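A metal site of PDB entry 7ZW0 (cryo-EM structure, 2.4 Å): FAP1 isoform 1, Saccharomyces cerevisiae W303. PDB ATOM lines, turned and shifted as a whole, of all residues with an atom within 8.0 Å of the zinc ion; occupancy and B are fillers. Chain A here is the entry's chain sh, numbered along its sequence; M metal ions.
N of Cys 114 sits at hydrogen-bond distance from O of Tyr 119 (2.7 Å). N of Arg 89 sits close to SG of Cys 87 (3.4 Å). The side-chain sulfur of Cys 84 sits close to the backbone NH of Arg 86, at 3.5 Å.
Four residues have an atom within 4 Å of the zinc ion: Cys 84, Cys 87, Cys 114 and Cys 117. The nearest printed residue that does not touch the zinc ion is Phe 91 (4.5 Å).
The zinc ion is bound by the side-chain sulfur (SG) of Cys 114 (2.0 Å). The zinc ion is bound by SG of Cys 87 (2.4 Å). The zinc ion is bound by SG of Cys 84, at 2.5 Å. The zinc ion is bound by the side-chain sulfur (SG) of Cys 117, 2.6 Å away. The zinc ion has four donor atoms within binding distance.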
ATOM      1  N   MET A  69       3.009  16.234 -29.843  1.00  0.00           N
ATOM      2  CA  MET A  69       4.258  16.297 -29.082  1.00  0.00           C
ATOM      3  C   MET A  69       4.923  14.975 -28.729  1.00  0.00           C
ATOM      4  O   MET A  69       6.140  14.852 -28.846  1.00  0.00           O
ATOM      5  CB  MET A  69       4.054  17.133 -27.818  1.00  0.00           C
ATOM      6  CG  MET A  69       3.708  18.581 -28.104  1.00  0.00           C
ATOM      7  SD  MET A  69       3.639  19.619 -26.627  1.00  0.00           S
ATOM      8  CE  MET A  69       5.333  19.514 -26.061  1.00  0.00           C
ATOM      9  N   PHE A  82      -6.003  15.800 -28.501  1.00  0.00           N
ATOM     10  CA  PHE A  82      -6.311  15.975 -27.074  1.00  0.00           C
ATOM     11  C   PHE A  82      -5.959  17.392 -26.614  1.00  0.00           C
ATOM     12  O   PHE A  82      -4.886  17.895 -26.955  1.00  0.00           O
ATOM     13  CB  PHE A  82      -5.548  14.975 -26.232  1.00  0.00           C
ATOM     14  CG  PHE A  82      -5.762  15.147 -24.753  1.00  0.00           C
ATOM     15  CD1 PHE A  82      -6.931  14.708 -24.164  1.00  0.00           C
ATOM     16  CD2 PHE A  82      -4.795  15.731 -23.962  1.00  0.00           C
ATOM     17  CE1 PHE A  82      -7.143  14.863 -22.802  1.00  0.00           C
ATOM     18  CE2 PHE A  82      -4.994  15.902 -22.609  1.00  0.00           C
ATOM     19  CZ  PHE A  82      -6.163  15.458 -22.028  1.00  0.00           C
ATOM     20  N   ALA A  83      -6.844  18.033 -25.869  1.00  0.00           N
ATOM     21  CA  ALA A  83      -6.605  19.408 -25.448  1.00  0.00           C
ATOM     22  C   ALA A  83      -6.500  19.545 -23.945  1.00  0.00           C
ATOM     23  O   ALA A  83      -7.283  18.953 -23.202  1.00  0.00           O
ATOM     24  CB  ALA A  83      -7.677  20.323 -25.998  1.00  0.00           C
ATOM     25  N   CYS A  84      -5.543  20.334 -23.484  1.00  0.00           N
ATOM     26  CA  CYS A  84      -5.407  20.579 -22.055  1.00  0.00           C
ATOM     27  C   CYS A  84      -5.636  22.051 -21.816  1.00  0.00           C
ATOM     28  O   CYS A  84      -5.071  22.875 -22.519  1.00  0.00           O
ATOM     29  CB  CYS A  84      -4.023  20.172 -21.546  1.00  0.00           C
ATOM     30  SG  CYS A  84      -3.688  20.659 -19.844  1.00  0.00           S
ATOM     31  N   LYS A  85      -6.456  22.396 -20.836  1.00  0.00           N
ATOM     32  CA  LYS A  85      -6.780  23.796 -20.616  1.00  0.00           C
ATOM     33  C   LYS A  85      -5.559  24.609 -20.239  1.00  0.00           C
ATOM     34  O   LYS A  85      -5.398  25.734 -20.684  1.00  0.00           O
ATOM     35  CB  LYS A  85      -7.860  23.935 -19.528  1.00  0.00           C
ATOM     36  CG  LYS A  85      -9.284  23.633 -19.993  1.00  0.00           C
ATOM     37  CD  LYS A  85      -9.585  22.139 -20.023  1.00  0.00           C
ATOM     38  CE  LYS A  85      -9.686  21.618 -21.438  1.00  0.00           C
ATOM     39  NZ  LYS A  85      -9.651  20.130 -21.480  1.00  0.00           N
ATOM     40  N   ARG A  86      -4.683  24.039 -19.425  1.00  0.00           N
ATOM     41  CA  ARG A  86      -3.522  24.784 -18.964  1.00  0.00           C
ATOM     42  C   ARG A  86      -2.585  25.186 -20.110  1.00  0.00           C
ATOM     43  O   ARG A  86      -2.117  26.327 -20.156  1.00  0.00           O
ATOM     44  CB  ARG A  86      -2.768  23.987 -17.893  1.00  0.00           C
ATOM     45  CG  ARG A  86      -1.815  24.830 -17.058  1.00  0.00           C
ATOM     46  CD  ARG A  86      -2.565  25.889 -16.274  1.00  0.00           C
ATOM     47  NE  ARG A  86      -1.685  26.955 -15.805  1.00  0.00           N
ATOM     48  CZ  ARG A  86      -1.454  28.084 -16.470  1.00  0.00           C
ATOM     49  NH1 ARG A  86      -2.047  28.299 -17.633  1.00  0.00           N
ATOM     50  NH2 ARG A  86      -0.629  28.998 -15.973  1.00  0.00           N
ATOM     51  N   CYS A  87      -2.328  24.272 -21.036  1.00  0.00           N
ATOM     52  CA  CYS A  87      -1.445  24.588 -22.157  1.00  0.00           C
ATOM     53  C   CYS A  87      -2.161  24.944 -23.443  1.00  0.00           C
ATOM     54  O   CYS A  87      -1.522  25.434 -24.375  1.00  0.00           O
ATOM     55  CB  CYS A  87      -0.527  23.408 -22.445  1.00  0.00           C
ATOM     56  SG  CYS A  87      -1.376  21.990 -23.170  1.00  0.00           S
ATOM     57  N   TYR A  88      -3.466  24.743 -23.498  1.00  0.00           N
ATOM     58  CA  TYR A  88      -4.215  24.958 -24.737  1.00  0.00           C
ATOM     59  C   TYR A  88      -3.445  24.515 -25.975  1.00  0.00           C
ATOM     60  O   TYR A  88      -3.373  25.246 -26.970  1.00  0.00           O
ATOM     61  CB  TYR A  88      -4.720  26.398 -24.851  1.00  0.00           C
ATOM     62  CG  TYR A  88      -5.992  26.613 -24.070  1.00  0.00           C
ATOM     63  CD1 TYR A  88      -7.070  25.752 -24.239  1.00  0.00           C
ATOM     64  CD2 TYR A  88      -6.120  27.665 -23.185  1.00  0.00           C
ATOM     65  CE1 TYR A  88      -8.241  25.936 -23.528  1.00  0.00           C
ATOM     66  CE2 TYR A  88      -7.283  27.857 -22.467  1.00  0.00           C
ATOM     67  CZ  TYR A  88      -8.342  26.981 -22.638  1.00  0.00           C
ATOM     68  OH  TYR A  88      -9.504  27.169 -21.929  1.00  0.00           O
ATOM     69  N   ARG A  89      -2.880  23.314 -25.929  1.00  0.00           N
ATOM     70  CA  ARG A  89      -2.129  22.785 -27.047  1.00  0.00           C
ATOM     71  C   ARG A  89      -2.700  21.412 -27.380  1.00  0.00           C
ATOM     72  O   ARG A  89      -3.303  20.768 -26.518  1.00  0.00           O
ATOM     73  CB  ARG A  89      -0.644  22.710 -26.671  1.00  0.00           C
ATOM     74  CG  ARG A  89       0.222  21.738 -27.455  1.00  0.00           C
ATOM     75  CD  ARG A  89       1.084  22.446 -28.482  1.00  0.00           C
ATOM     76  NE  ARG A  89       1.811  21.499 -29.321  1.00  0.00           N
ATOM     77  CZ  ARG A  89       2.703  21.845 -30.251  1.00  0.00           C
ATOM     78  NH1 ARG A  89       2.987  23.124 -30.444  1.00  0.00           N
ATOM     79  NH2 ARG A  89       3.303  20.912 -30.977  1.00  0.00           N
ATOM     80  N   VAL A  90      -2.533  20.949 -28.610  1.00  0.00           N
ATOM     81  CA  VAL A  90      -3.099  19.667 -29.019  1.00  0.00           C
ATOM     82  C   VAL A  90      -2.086  18.604 -29.430  1.00  0.00           C
ATOM     83  O   VAL A  90      -1.101  18.904 -30.119  1.00  0.00           O
ATOM     84  CB  VAL A  90      -4.168  19.868 -30.101  1.00  0.00           C
ATOM     85  CG1 VAL A  90      -4.287  18.677 -31.020  1.00  0.00           C
ATOM     86  CG2 VAL A  90      -5.496  20.181 -29.450  1.00  0.00           C
ATOM     87  N   PHE A  91      -2.282  17.371 -28.969  1.00  0.00           N
ATOM     88  CA  PHE A  91      -1.389  16.276 -29.331  1.00  0.00           C
ATOM     89  C   PHE A  91      -2.284  15.171 -29.847  1.00  0.00           C
ATOM     90  O   PHE A  91      -3.495  15.248 -29.702  1.00  0.00           O
ATOM     91  CB  PHE A  91      -0.630  15.780 -28.101  1.00  0.00           C
ATOM     92  CG  PHE A  91      -0.672  16.723 -26.939  1.00  0.00           C
ATOM     93  CD1 PHE A  91      -1.722  16.668 -26.025  1.00  0.00           C
ATOM     94  CD2 PHE A  91       0.326  17.664 -26.751  1.00  0.00           C
ATOM     95  CE1 PHE A  91      -1.764  17.543 -24.950  1.00  0.00           C
ATOM     96  CE2 PHE A  91       0.289  18.527 -25.681  1.00  0.00           C
ATOM     97  CZ  PHE A  91      -0.765  18.474 -24.780  1.00  0.00           C
ATOM     98  N   ILE A  96      -0.781  10.900 -26.553  1.00  0.00           N
ATOM     99  CA  ILE A  96      -0.754  11.502 -25.234  1.00  0.00           C
ATOM    100  C   ILE A  96      -1.226  10.510 -24.161  1.00  0.00           C
ATOM    101  O   ILE A  96      -0.782  10.590 -23.016  1.00  0.00           O
ATOM    102  CB  ILE A  96      -1.560  12.821 -25.186  1.00  0.00           C
ATOM    103  CG1 ILE A  96      -1.093  13.702 -24.023  1.00  0.00           C
ATOM    104  CG2 ILE A  96      -3.058  12.570 -25.058  1.00  0.00           C
ATOM    105  CD1 ILE A  96       0.357  14.115 -24.120  1.00  0.00           C
ATOM    106  N   TRP A 112      -0.977  11.649 -14.293  1.00  0.00           N
ATOM    107  CA  TRP A 112      -0.505  11.919 -15.649  1.00  0.00           C
ATOM    108  C   TRP A 112      -0.024  13.367 -15.817  1.00  0.00           C
ATOM    109  O   TRP A 112      -0.544  14.262 -15.170  1.00  0.00           O
ATOM    110  CB  TRP A 112      -1.602  11.584 -16.661  1.00  0.00           C
ATOM    111  CG  TRP A 112      -2.342  12.758 -17.198  1.00  0.00           C
ATOM    112  CD1 TRP A 112      -3.395  13.401 -16.624  1.00  0.00           C
ATOM    113  CD2 TRP A 112      -2.089  13.437 -18.444  1.00  0.00           C
ATOM    114  NE1 TRP A 112      -3.811  14.430 -17.432  1.00  0.00           N
ATOM    115  CE2 TRP A 112      -3.021  14.474 -18.549  1.00  0.00           C
ATOM    116  CE3 TRP A 112      -1.156  13.256 -19.469  1.00  0.00           C
ATOM    117  CZ2 TRP A 112      -3.057  15.333 -19.636  1.00  0.00           C
ATOM    118  CZ3 TRP A 112      -1.196  14.109 -20.540  1.00  0.00           C
ATOM    119  CH2 TRP A 112      -2.133  15.139 -20.630  1.00  0.00           C
ATOM    120  N   LYS A 113       0.958  13.604 -16.690  1.00  0.00           N
ATOM    121  CA  LYS A 113       1.510  14.969 -16.829  1.00  0.00           C
ATOM    122  C   LYS A 113       1.373  15.523 -18.240  1.00  0.00           C
ATOM    123  O   LYS A 113       1.602  14.809 -19.204  1.00  0.00           O
ATOM    124  CB  LYS A 113       2.985  14.980 -16.411  1.00  0.00           C
ATOM    125  CG  LYS A 113       3.576  16.377 -16.277  1.00  0.00           C
ATOM    126  CD  LYS A 113       4.832  16.352 -15.429  1.00  0.00           C
ATOM    127  CE  LYS A 113       5.198  17.756 -14.984  1.00  0.00           C
ATOM    128  NZ  LYS A 113       6.331  17.743 -14.009  1.00  0.00           N
ATOM    129  N   CYS A 114       1.011  16.784 -18.358  1.00  0.00           N
ATOM    130  CA  CYS A 114       0.915  17.402 -19.666  1.00  0.00           C
ATOM    131  C   CYS A 114       2.204  18.128 -19.977  1.00  0.00           C
ATOM    132  O   CYS A 114       2.577  19.049 -19.260  1.00  0.00           O
ATOM    133  CB  CYS A 114      -0.257  18.372 -19.718  1.00  0.00           C
ATOM    134  SG  CYS A 114      -0.477  19.134 -21.336  1.00  0.00           S
ATOM    135  N   PRO A 115       2.893  17.745 -21.056  1.00  0.00           N
ATOM    136  CA  PRO A 115       4.208  18.324 -21.373  1.00  0.00           C
ATOM    137  C   PRO A 115       4.273  19.810 -21.721  1.00  0.00           C
ATOM    138  O   PRO A 115       5.200  20.474 -21.258  1.00  0.00           O
ATOM    139  CB  PRO A 115       4.665  17.525 -22.602  1.00  0.00           C
ATOM    140  CG  PRO A 115       3.799  16.300 -22.628  1.00  0.00           C
ATOM    141  CD  PRO A 115       2.493  16.722 -22.040  1.00  0.00           C
ATOM    142  N   ASN A 116       3.341  20.322 -22.504  1.00  0.00           N
ATOM    143  CA  ASN A 116       3.452  21.719 -22.936  1.00  0.00           C
ATOM    144  C   ASN A 116       3.391  22.696 -21.784  1.00  0.00           C
ATOM    145  O   ASN A 116       4.161  23.660 -21.736  1.00  0.00           O
ATOM    146  CB  ASN A 116       2.385  22.052 -23.980  1.00  0.00           C
ATOM    147  CG  ASN A 116       2.743  23.290 -24.796  1.00  0.00           C
ATOM    148  OD1 ASN A 116       3.831  23.364 -25.372  1.00  0.00           O
ATOM    149  ND2 ASN A 116       1.828  24.241 -24.862  1.00  0.00           N
ATOM    150  N   CYS A 117       2.493  22.463 -20.839  1.00  0.00           N
ATOM    151  CA  CYS A 117       2.419  23.315 -19.661  1.00  0.00           C
ATOM    152  C   CYS A 117       3.243  22.724 -18.545  1.00  0.00           C
ATOM    153  O   CYS A 117       3.297  23.297 -17.452  1.00  0.00           O
ATOM    154  CB  CYS A 117       0.975  23.485 -19.209  1.00  0.00           C
ATOM    155  SG  CYS A 117       0.031  21.956 -19.235  1.00  0.00           S
ATOM    156  N   TYR A 118       3.868  21.578 -18.797  1.00  0.00           N
ATOM    157  CA  TYR A 118       4.640  20.888 -17.765  1.00  0.00           C
ATOM    158  C   TYR A 118       3.773  20.829 -16.527  1.00  0.00           C
ATOM    159  O   TYR A 118       4.231  21.119 -15.424  1.00  0.00           O
ATOM    160  CB  TYR A 118       5.970  21.612 -17.493  1.00  0.00           C
ATOM    161  CG  TYR A 118       7.035  20.730 -16.905  1.00  0.00           C
ATOM    162  CD1 TYR A 118       7.491  19.603 -17.581  1.00  0.00           C
ATOM    163  CD2 TYR A 118       7.602  21.024 -15.671  1.00  0.00           C
ATOM    164  CE1 TYR A 118       8.464  18.794 -17.039  1.00  0.00           C
ATOM    165  CE2 TYR A 118       8.584  20.224 -15.123  1.00  0.00           C
ATOM    166  CZ  TYR A 118       9.017  19.109 -15.819  1.00  0.00           C
ATOM    167  OH  TYR A 118       9.998  18.304 -15.280  1.00  0.00           O
ATOM    168  N   TYR A 119       2.509  20.460 -16.703  1.00  0.00           N
ATOM    169  CA  TYR A 119       1.579  20.451 -15.578  1.00  0.00           C
ATOM    170  C   TYR A 119       0.986  19.088 -15.372  1.00  0.00           C
ATOM    171  O   TYR A 119       0.462  18.485 -16.306  1.00  0.00           O
ATOM    172  CB  TYR A 119       0.508  21.530 -15.795  1.00  0.00           C
ATOM    173  CG  TYR A 119      -0.929  21.155 -15.476  1.00  0.00           C
ATOM    174  CD1 TYR A 119      -1.756  20.596 -16.437  1.00  0.00           C
ATOM    175  CD2 TYR A 119      -1.471  21.417 -14.226  1.00  0.00           C
ATOM    176  CE1 TYR A 119      -3.064  20.264 -16.161  1.00  0.00           C
ATOM    177  CE2 TYR A 119      -2.780  21.090 -13.941  1.00  0.00           C
ATOM    178  CZ  TYR A 119      -3.566  20.516 -14.904  1.00  0.00           C
ATOM    179  OH  TYR A 119      -4.874  20.184 -14.627  1.00  0.00           O
ATOM    180  N   VAL A 120       1.093  18.567 -14.156  1.00  0.00           N
ATOM    181  CA  VAL A 120       0.499  17.272 -13.863  1.00  0.00           C
ATOM    182  C   VAL A 120      -0.992  17.396 -13.653  1.00  0.00           C
ATOM    183  O   VAL A 120      -1.466  18.381 -13.104  1.00  0.00           O
ATOM    184  CB  VAL A 120       1.130  16.658 -12.604  1.00  0.00           C
ATOM    185  CG1 VAL A 120       1.757  15.307 -12.931  1.00  0.00           C
ATOM    186  CG2 VAL A 120       2.167  17.595 -12.029  1.00  0.00           C
ATOM    187  N   SER A 121      -1.742  16.392 -14.071  1.00  0.00           N
ATOM    188  CA  SER A 121      -3.186  16.380 -13.850  1.00  0.00           C
ATOM    189  C   SER A 121      -3.535  15.029 -13.269  1.00  0.00           C
ATOM    190  O   SER A 121      -2.709  14.110 -13.319  1.00  0.00           O
ATOM    191  CB  SER A 121      -3.958  16.688 -15.133  1.00  0.00           C
ATOM    192  OG  SER A 121      -5.354  16.775 -14.886  1.00  0.00           O
HETATM  193 ZN    ZN M   1      -1.487  20.893 -21.056  1.00  0.00          ZN
